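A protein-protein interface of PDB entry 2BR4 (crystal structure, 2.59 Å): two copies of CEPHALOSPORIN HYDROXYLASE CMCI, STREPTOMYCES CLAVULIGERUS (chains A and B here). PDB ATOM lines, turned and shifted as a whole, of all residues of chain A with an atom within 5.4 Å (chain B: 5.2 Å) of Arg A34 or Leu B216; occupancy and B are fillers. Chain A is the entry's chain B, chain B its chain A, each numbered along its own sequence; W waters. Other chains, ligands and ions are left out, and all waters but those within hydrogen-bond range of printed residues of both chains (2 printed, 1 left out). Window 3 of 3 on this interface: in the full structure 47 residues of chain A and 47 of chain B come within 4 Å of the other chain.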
ATOM      1  N   PRO A  27      20.614  -5.561  -2.640  1.00  0.00           N
ATOM      2  CA  PRO A  27      19.225  -5.560  -2.181  1.00  0.00           C
ATOM      3  C   PRO A  27      18.439  -4.419  -2.801  1.00  0.00           C
ATOM      4  O   PRO A  27      18.998  -3.403  -3.213  1.00  0.00           O
ATOM      5  CB  PRO A  27      19.345  -5.363  -0.668  1.00  0.00           C
ATOM      6  CG  PRO A  27      20.703  -5.824  -0.319  1.00  0.00           C
ATOM      7  CD  PRO A  27      21.559  -5.485  -1.513  1.00  0.00           C
ATOM      8  N   LEU A  29      15.150  -1.982  -2.060  1.00  0.00           N
ATOM      9  CA  LEU A  29      14.187  -1.482  -1.085  1.00  0.00           C
ATOM     10  C   LEU A  29      12.802  -1.502  -1.733  1.00  0.00           C
ATOM     11  O   LEU A  29      12.637  -1.079  -2.885  1.00  0.00           O
ATOM     12  CB  LEU A  29      14.559  -0.067  -0.606  1.00  0.00           C
ATOM     13  CG  LEU A  29      15.459   0.144   0.635  1.00  0.00           C
ATOM     14  CD1 LEU A  29      15.848  -1.152   1.332  1.00  0.00           C
ATOM     15  CD2 LEU A  29      16.712   0.968   0.300  1.00  0.00           C
ATOM     16  N   ARG A  32      10.271   1.585   1.177  1.00  0.00           N
ATOM     17  CA  ARG A  32      10.828   2.876   1.588  1.00  0.00           C
ATOM     18  C   ARG A  32      11.817   3.433   0.578  1.00  0.00           C
ATOM     19  O   ARG A  32      12.393   2.688  -0.212  1.00  0.00           O
ATOM     20  CB  ARG A  32      11.519   2.758   2.946  1.00  0.00           C
ATOM     21  CG  ARG A  32      12.672   1.766   2.987  1.00  0.00           C
ATOM     22  CD  ARG A  32      12.310   0.467   3.662  1.00  0.00           C
ATOM     23  NE  ARG A  32      13.020   0.270   4.914  1.00  0.00           N
ATOM     24  CZ  ARG A  32      12.671  -0.604   5.856  1.00  0.00           C
ATOM     25  NH1 ARG A  32      11.596  -1.372   5.718  1.00  0.00           N
ATOM     26  NH2 ARG A  32      13.406  -0.707   6.955  1.00  0.00           N
ATOM     27  N   PRO A  33      12.037   4.741   0.617  1.00  0.00           N
ATOM     28  CA  PRO A  33      13.057   5.348  -0.227  1.00  0.00           C
ATOM     29  C   PRO A  33      14.405   5.057   0.365  1.00  0.00           C
ATOM     30  O   PRO A  33      14.507   4.764   1.563  1.00  0.00           O
ATOM     31  CB  PRO A  33      12.760   6.843  -0.124  1.00  0.00           C
ATOM     32  CG  PRO A  33      12.131   7.010   1.209  1.00  0.00           C
ATOM     33  CD  PRO A  33      11.362   5.741   1.463  1.00  0.00           C
ATOM     34  N   ARG A  34      15.436   5.140  -0.461  1.00  0.00           N
ATOM     35  CA  ARG A  34      16.777   4.931   0.026  1.00  0.00           C
ATOM     36  C   ARG A  34      17.255   6.109   0.872  1.00  0.00           C
ATOM     37  O   ARG A  34      18.021   5.911   1.804  1.00  0.00           O
ATOM     38  CB  ARG A  34      17.741   4.679  -1.127  1.00  0.00           C
ATOM     39  CG  ARG A  34      19.125   4.323  -0.643  1.00  0.00           C
ATOM     40  CD  ARG A  34      20.030   3.731  -1.681  1.00  0.00           C
ATOM     41  NE  ARG A  34      21.401   3.695  -1.180  1.00  0.00           N
ATOM     42  CZ  ARG A  34      22.394   3.058  -1.769  1.00  0.00           C
ATOM     43  NH1 ARG A  34      22.198   2.408  -2.903  1.00  0.00           N
ATOM     44  NH2 ARG A  34      23.600   3.088  -1.225  1.00  0.00           N
ATOM     45  N   ASP A  35      16.803   7.323   0.549  1.00  0.00           N
ATOM     46  CA  ASP A  35      17.255   8.529   1.227  1.00  0.00           C
ATOM     47  C   ASP A  35      16.175   9.067   2.126  1.00  0.00           C
ATOM     48  O   ASP A  35      15.321   9.834   1.678  1.00  0.00           O
ATOM     49  CB  ASP A  35      17.628   9.599   0.212  1.00  0.00           C
ATOM     50  CG  ASP A  35      18.877   9.256  -0.560  1.00  0.00           C
ATOM     51  OD1 ASP A  35      19.923   8.933   0.056  1.00  0.00           O
ATOM     52  OD2 ASP A  35      18.904   9.295  -1.801  1.00  0.00           O
ATOM     53  N   TRP A  36      16.203   8.678   3.397  1.00  0.00           N
ATOM     54  CA  TRP A  36      15.218   9.163   4.358  1.00  0.00           C
ATOM     55  C   TRP A  36      15.511  10.614   4.763  1.00  0.00           C
ATOM     56  O   TRP A  36      16.654  10.946   5.075  1.00  0.00           O
ATOM     57  CB  TRP A  36      15.182   8.269   5.601  1.00  0.00           C
ATOM     58  CG  TRP A  36      13.895   8.382   6.334  1.00  0.00           C
ATOM     59  CD1 TRP A  36      13.609   9.244   7.345  1.00  0.00           C
ATOM     60  CD2 TRP A  36      12.698   7.638   6.092  1.00  0.00           C
ATOM     61  NE1 TRP A  36      12.311   9.073   7.761  1.00  0.00           N
ATOM     62  CE2 TRP A  36      11.725   8.096   7.003  1.00  0.00           C
ATOM     63  CE3 TRP A  36      12.346   6.616   5.202  1.00  0.00           C
ATOM     64  CZ2 TRP A  36      10.429   7.571   7.055  1.00  0.00           C
ATOM     65  CZ3 TRP A  36      11.046   6.104   5.243  1.00  0.00           C
ATOM     66  CH2 TRP A  36      10.112   6.580   6.170  1.00  0.00           C
ATOM     67  N   LEU A  48      15.263  -4.434   8.599  1.00  0.00           N
ATOM     68  CA  LEU A  48      16.376  -4.443   7.664  1.00  0.00           C
ATOM     69  C   LEU A  48      16.015  -3.789   6.327  1.00  0.00           C
ATOM     70  O   LEU A  48      16.832  -3.079   5.755  1.00  0.00           O
ATOM     71  CB  LEU A  48      16.869  -5.877   7.456  1.00  0.00           C
ATOM     72  CG  LEU A  48      18.130  -6.063   6.618  1.00  0.00           C
ATOM     73  CD1 LEU A  48      19.325  -5.371   7.271  1.00  0.00           C
ATOM     74  CD2 LEU A  48      18.422  -7.549   6.401  1.00  0.00           C
ATOM     75  N   TYR A  50      14.889  -5.639   3.675  1.00  0.00           N
ATOM     76  CA  TYR A  50      14.947  -6.723   2.686  1.00  0.00           C
ATOM     77  C   TYR A  50      15.170  -8.083   3.366  1.00  0.00           C
ATOM     78  O   TYR A  50      15.426  -8.167   4.563  1.00  0.00           O
ATOM     79  CB  TYR A  50      16.036  -6.463   1.640  1.00  0.00           C
ATOM     80  CG  TYR A  50      17.402  -6.167   2.218  1.00  0.00           C
ATOM     81  CD1 TYR A  50      18.330  -7.188   2.412  1.00  0.00           C
ATOM     82  CD2 TYR A  50      17.775  -4.868   2.556  1.00  0.00           C
ATOM     83  CE1 TYR A  50      19.586  -6.932   2.940  1.00  0.00           C
ATOM     84  CE2 TYR A  50      19.033  -4.599   3.086  1.00  0.00           C
ATOM     85  CZ  TYR A  50      19.934  -5.638   3.273  1.00  0.00           C
ATOM     86  OH  TYR A  50      21.182  -5.394   3.793  1.00  0.00           O
ATOM     87  N   GLU B  79      30.352  -0.384  -3.699  1.00  0.00           N
ATOM     88  CA  GLU B  79      29.444   0.440  -4.480  1.00  0.00           C
ATOM     89  C   GLU B  79      30.009   1.859  -4.757  1.00  0.00           C
ATOM     90  O   GLU B  79      29.986   2.343  -5.888  1.00  0.00           O
ATOM     91  CB  GLU B  79      28.116   0.522  -3.726  1.00  0.00           C
ATOM     92  CG  GLU B  79      27.173   1.616  -4.193  1.00  0.00           C
ATOM     93  CD  GLU B  79      25.958   1.710  -3.310  1.00  0.00           C
ATOM     94  OE1 GLU B  79      26.114   1.985  -2.105  1.00  0.00           O
ATOM     95  OE2 GLU B  79      24.850   1.489  -3.819  1.00  0.00           O
ATOM     96  N   TYR B 182      29.724  10.138   2.313  1.00  0.00           N
ATOM     97  CA  TYR B 182      29.093   9.687   3.541  1.00  0.00           C
ATOM     98  C   TYR B 182      29.660  10.390   4.777  1.00  0.00           C
ATOM     99  O   TYR B 182      30.833  10.720   4.827  1.00  0.00           O
ATOM    100  CB  TYR B 182      29.260   8.174   3.687  1.00  0.00           C
ATOM    101  CG  TYR B 182      28.313   7.377   2.822  1.00  0.00           C
ATOM    102  CD1 TYR B 182      28.568   7.193   1.468  1.00  0.00           C
ATOM    103  CD2 TYR B 182      27.167   6.807   3.357  1.00  0.00           C
ATOM    104  CE1 TYR B 182      27.705   6.466   0.677  1.00  0.00           C
ATOM    105  CE2 TYR B 182      26.299   6.080   2.572  1.00  0.00           C
ATOM    106  CZ  TYR B 182      26.565   5.915   1.233  1.00  0.00           C
ATOM    107  OH  TYR B 182      25.699   5.193   0.442  1.00  0.00           O
ATOM    108  N   SER B 212      20.991  13.018   4.059  1.00  0.00           N
ATOM    109  CA  SER B 212      19.901  12.055   4.202  1.00  0.00           C
ATOM    110  C   SER B 212      20.424  10.801   4.897  1.00  0.00           C
ATOM    111  O   SER B 212      21.626  10.599   4.987  1.00  0.00           O
ATOM    112  CB  SER B 212      19.339  11.659   2.837  1.00  0.00           C
ATOM    113  OG  SER B 212      20.068  10.565   2.278  1.00  0.00           O
ATOM    114  N   MET B 213      19.513   9.959   5.373  1.00  0.00           N
ATOM    115  CA  MET B 213      19.876   8.706   6.011  1.00  0.00           C
ATOM    116  C   MET B 213      19.749   7.579   4.995  1.00  0.00           C
ATOM    117  O   MET B 213      18.689   7.363   4.425  1.00  0.00           O
ATOM    118  CB  MET B 213      19.002   8.435   7.238  1.00  0.00           C
ATOM    119  CG  MET B 213      19.259   7.076   7.878  1.00  0.00           C
ATOM    120  SD  MET B 213      18.641   6.928   9.565  1.00  0.00           S
ATOM    121  CE  MET B 213      16.843   7.215   9.294  1.00  0.00           C
ATOM    122  N   ASP B 214      20.842   6.865   4.768  1.00  0.00           N
ATOM    123  CA  ASP B 214      20.885   5.843   3.745  1.00  0.00           C
ATOM    124  C   ASP B 214      20.250   4.566   4.286  1.00  0.00           C
ATOM    125  O   ASP B 214      20.857   3.845   5.078  1.00  0.00           O
ATOM    126  CB  ASP B 214      22.333   5.615   3.320  1.00  0.00           C
ATOM    127  CG  ASP B 214      22.448   4.828   2.045  1.00  0.00           C
ATOM    128  OD1 ASP B 214      21.500   4.091   1.684  1.00  0.00           O
ATOM    129  OD2 ASP B 214      23.477   4.879   1.344  1.00  0.00           O
ATOM    130  N   MET B 215      19.027   4.294   3.841  1.00  0.00           N
ATOM    131  CA  MET B 215      18.234   3.180   4.345  1.00  0.00           C
ATOM    132  C   MET B 215      18.632   1.821   3.762  1.00  0.00           C
ATOM    133  O   MET B 215      17.991   0.822   4.063  1.00  0.00           O
ATOM    134  CB  MET B 215      16.750   3.428   4.076  1.00  0.00           C
ATOM    135  CG  MET B 215      16.207   4.732   4.670  1.00  0.00           C
ATOM    136  SD  MET B 215      16.333   4.778   6.461  1.00  0.00           S
ATOM    137  CE  MET B 215      15.107   3.496   6.888  1.00  0.00           C
ATOM    138  N   LEU B 216      19.675   1.781   2.931  1.00  0.00           N
ATOM    139  CA  LEU B 216      20.262   0.510   2.501  1.00  0.00           C
ATOM    140  C   LEU B 216      21.166  -0.052   3.598  1.00  0.00           C
ATOM    141  O   LEU B 216      21.191  -1.259   3.831  1.00  0.00           O
ATOM    142  CB  LEU B 216      21.074   0.683   1.210  1.00  0.00           C
ATOM    143  CG  LEU B 216      20.936  -0.349   0.077  1.00  0.00           C
ATOM    144  CD1 LEU B 216      22.272  -0.562  -0.635  1.00  0.00           C
ATOM    145  CD2 LEU B 216      20.379  -1.673   0.544  1.00  0.00           C
ATOM    146  N   TYR B 217      21.904   0.831   4.260  1.00  0.00           N
ATOM    147  CA  TYR B 217      22.911   0.436   5.231  1.00  0.00           C
ATOM    148  C   TYR B 217      22.571   0.809   6.672  1.00  0.00           C
ATOM    149  O   TYR B 217      23.203   0.324   7.594  1.00  0.00           O
ATOM    150  CB  TYR B 217      24.247   1.088   4.864  1.00  0.00           C
ATOM    151  CG  TYR B 217      24.733   0.782   3.463  1.00  0.00           C
ATOM    152  CD1 TYR B 217      25.176   1.798   2.629  1.00  0.00           C
ATOM    153  CD2 TYR B 217      24.760  -0.527   2.978  1.00  0.00           C
ATOM    154  CE1 TYR B 217      25.626   1.520   1.338  1.00  0.00           C
ATOM    155  CE2 TYR B 217      25.203  -0.814   1.704  1.00  0.00           C
ATOM    156  CZ  TYR B 217      25.634   0.209   0.883  1.00  0.00           C
ATOM    157  OH  TYR B 217      26.078  -0.056  -0.394  1.00  0.00           O
ATOM    158  N   ALA B 218      21.578   1.666   6.873  1.00  0.00           N
ATOM    159  CA  ALA B 218      21.332   2.243   8.194  1.00  0.00           C
ATOM    160  C   ALA B 218      20.829   1.229   9.204  1.00  0.00           C
ATOM    161  O   ALA B 218      21.127   1.355  10.386  1.00  0.00           O
ATOM    162  CB  ALA B 218      20.358   3.408   8.100  1.00  0.00           C
ATOM    163  N   ALA B 220      21.489  -2.159   9.004  1.00  0.00           N
ATOM    164  CA  ALA B 220      22.160  -3.427   8.704  1.00  0.00           C
ATOM    165  C   ALA B 220      23.169  -3.861   9.764  1.00  0.00           C
ATOM    166  O   ALA B 220      23.582  -5.017   9.789  1.00  0.00           O
ATOM    167  CB  ALA B 220      22.827  -3.351   7.352  1.00  0.00           C
ATOM    168  N   ARG B 230      24.500  10.456   4.075  1.00  0.00           N
ATOM    169  CA  ARG B 230      25.236  10.910   2.904  1.00  0.00           C
ATOM    170  C   ARG B 230      24.749  12.273   2.405  1.00  0.00           C
ATOM    171  O   ARG B 230      23.633  12.689   2.685  1.00  0.00           O
ATOM    172  CB  ARG B 230      25.220   9.852   1.787  1.00  0.00           C
ATOM    173  CG  ARG B 230      23.872   9.509   1.187  1.00  0.00           C
ATOM    174  CD  ARG B 230      23.965   8.435   0.110  1.00  0.00           C
ATOM    175  NE  ARG B 230      22.694   8.181  -0.571  1.00  0.00           N
ATOM    176  CZ  ARG B 230      22.520   7.260  -1.526  1.00  0.00           C
ATOM    177  NH1 ARG B 230      23.525   6.504  -1.935  1.00  0.00           N
ATOM    178  NH2 ARG B 230      21.330   7.089  -2.085  1.00  0.00           N
HETATM  179  O   HOH W   1      16.160  -0.245   5.763  1.00  0.00           O
HETATM  180  O   HOH W   2      22.444  -3.199   2.860  1.00  0.00           O
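OE1 of Glu B79 sits at hydrogen-bond distance from OH of Tyr B217.
The side-chain hydroxyl (OH) of Tyr B182 lies within hydrogen-bond range of the side-chain carboxylate (OD2) of Asp B214.
NH1 of Arg B230 lies within hydrogen-bond range of OH of Tyr B182.
The backbone carbonyl oxygen (O) of Arg B230 sits at hydrogen-bond distance from the backbone NH (N) of Ser B212 (3.0 Å).
The backbone NH (N) of Leu B216 lies close to the side-chain carboxylate (OD1) of Asp B214, 3.2 Å away.
OD2 of Asp B214 lies within salt-bridge range of NH1 of Arg B230 (3.7 Å).
Leu A29 touches Met B215.
O of Pro A33 touches CG of Met B215, 3.5 Å away.
Leu B216 touches Arg A34 (CD1 to NH1, 3.7 Å).
Tyr B217 touches Arg A34 (CE1 to NH2, 3.6 Å).
Met B213 touches Asp A35.
O of Trp A36 touches CA of Ser B212, 3.5 Å away.
CB of Trp A36 touches SD of Met B215 (3.8 Å).
CD1 of Leu A48 touches CA of Ala B220, at 3.7 Å.
Of the 11 printed residues of chain B, 10 touch a printed residue of chain A.
Hydrophobic or aromatic side chains of chain A that line the printed part of chain B: Leu A29, Trp A36 and Leu A48.
Among the printed residues, 17 pairs touch across the chains.
Among the printed residues, Asp or Glu carboxylates within 4 Å of a Lys or Arg side-chain nitrogen of the other chain: Arg A34 with Glu B79 (2.9 Å), Arg A34 with Asp B214 (2.9 Å) and Asp A35 with Arg B230 (2.9 Å).
No position is printed for both chains.
Of the 17 pairs that touch across the chains among the printed residues, none has its exchanged pair printed and touching as well.
Water W2 lies within hydrogen-bond range of the backbone carbonyl oxygen of Leu B216 (2.5 Å) and the side-chain hydroxyl of Tyr A50 (2.7 Å).
Water W1 lies within hydrogen-bond range of O of Met B215 (2.7 Å), O of Leu A48 (2.9 Å) and NH2 of Arg A32 (3.0 Å).
Of the printed residues of chain B, Trp A36 touches Ser B212, Met B213 and Met B215.
Of the printed residues of chain A, Leu B216 touches Arg A34 (3.7 Å).
Printed residues of chain A within 4 Å of Arg B230: Arg A34 and Asp A35.
The nearest printed residue of chain A that does not touch Met B215 is Arg A32 (4.3 Å).
OE1 of Glu B79 is in salt-bridge range of NH2 of Arg A34.
OH of Tyr B182 sits at hydrogen-bond distance from NH2 of Arg A34.
OG of Ser B212 lies within hydrogen-bond range of OD1 of Asp A35, 2.8 Å away.
N of Trp A36 sits at hydrogen-bond distance from O of Met B213 (3.0 Å).
The side-chain carboxylate (OD1) of Asp B214 lies within salt-bridge range of the guanidinium group (NE) of Arg A34, at 2.9 Å.
N of Met B215 sits at hydrogen-bond distance from O of Arg A34, at 2.8 Å.
The side-chain carboxylate (OD1) of Asp A35 lies within salt-bridge range of the guanidinium group (NE) of Arg B230.
The backbone carbonyl oxygen (O) of Arg A34 lies close to the backbone carbonyl oxygen (O) of Met B213 (3.1 Å).
The guanidinium group (NH2) of Arg A34 sits close to the guanidinium group (NH1) of Arg B230 (3.5 Å).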
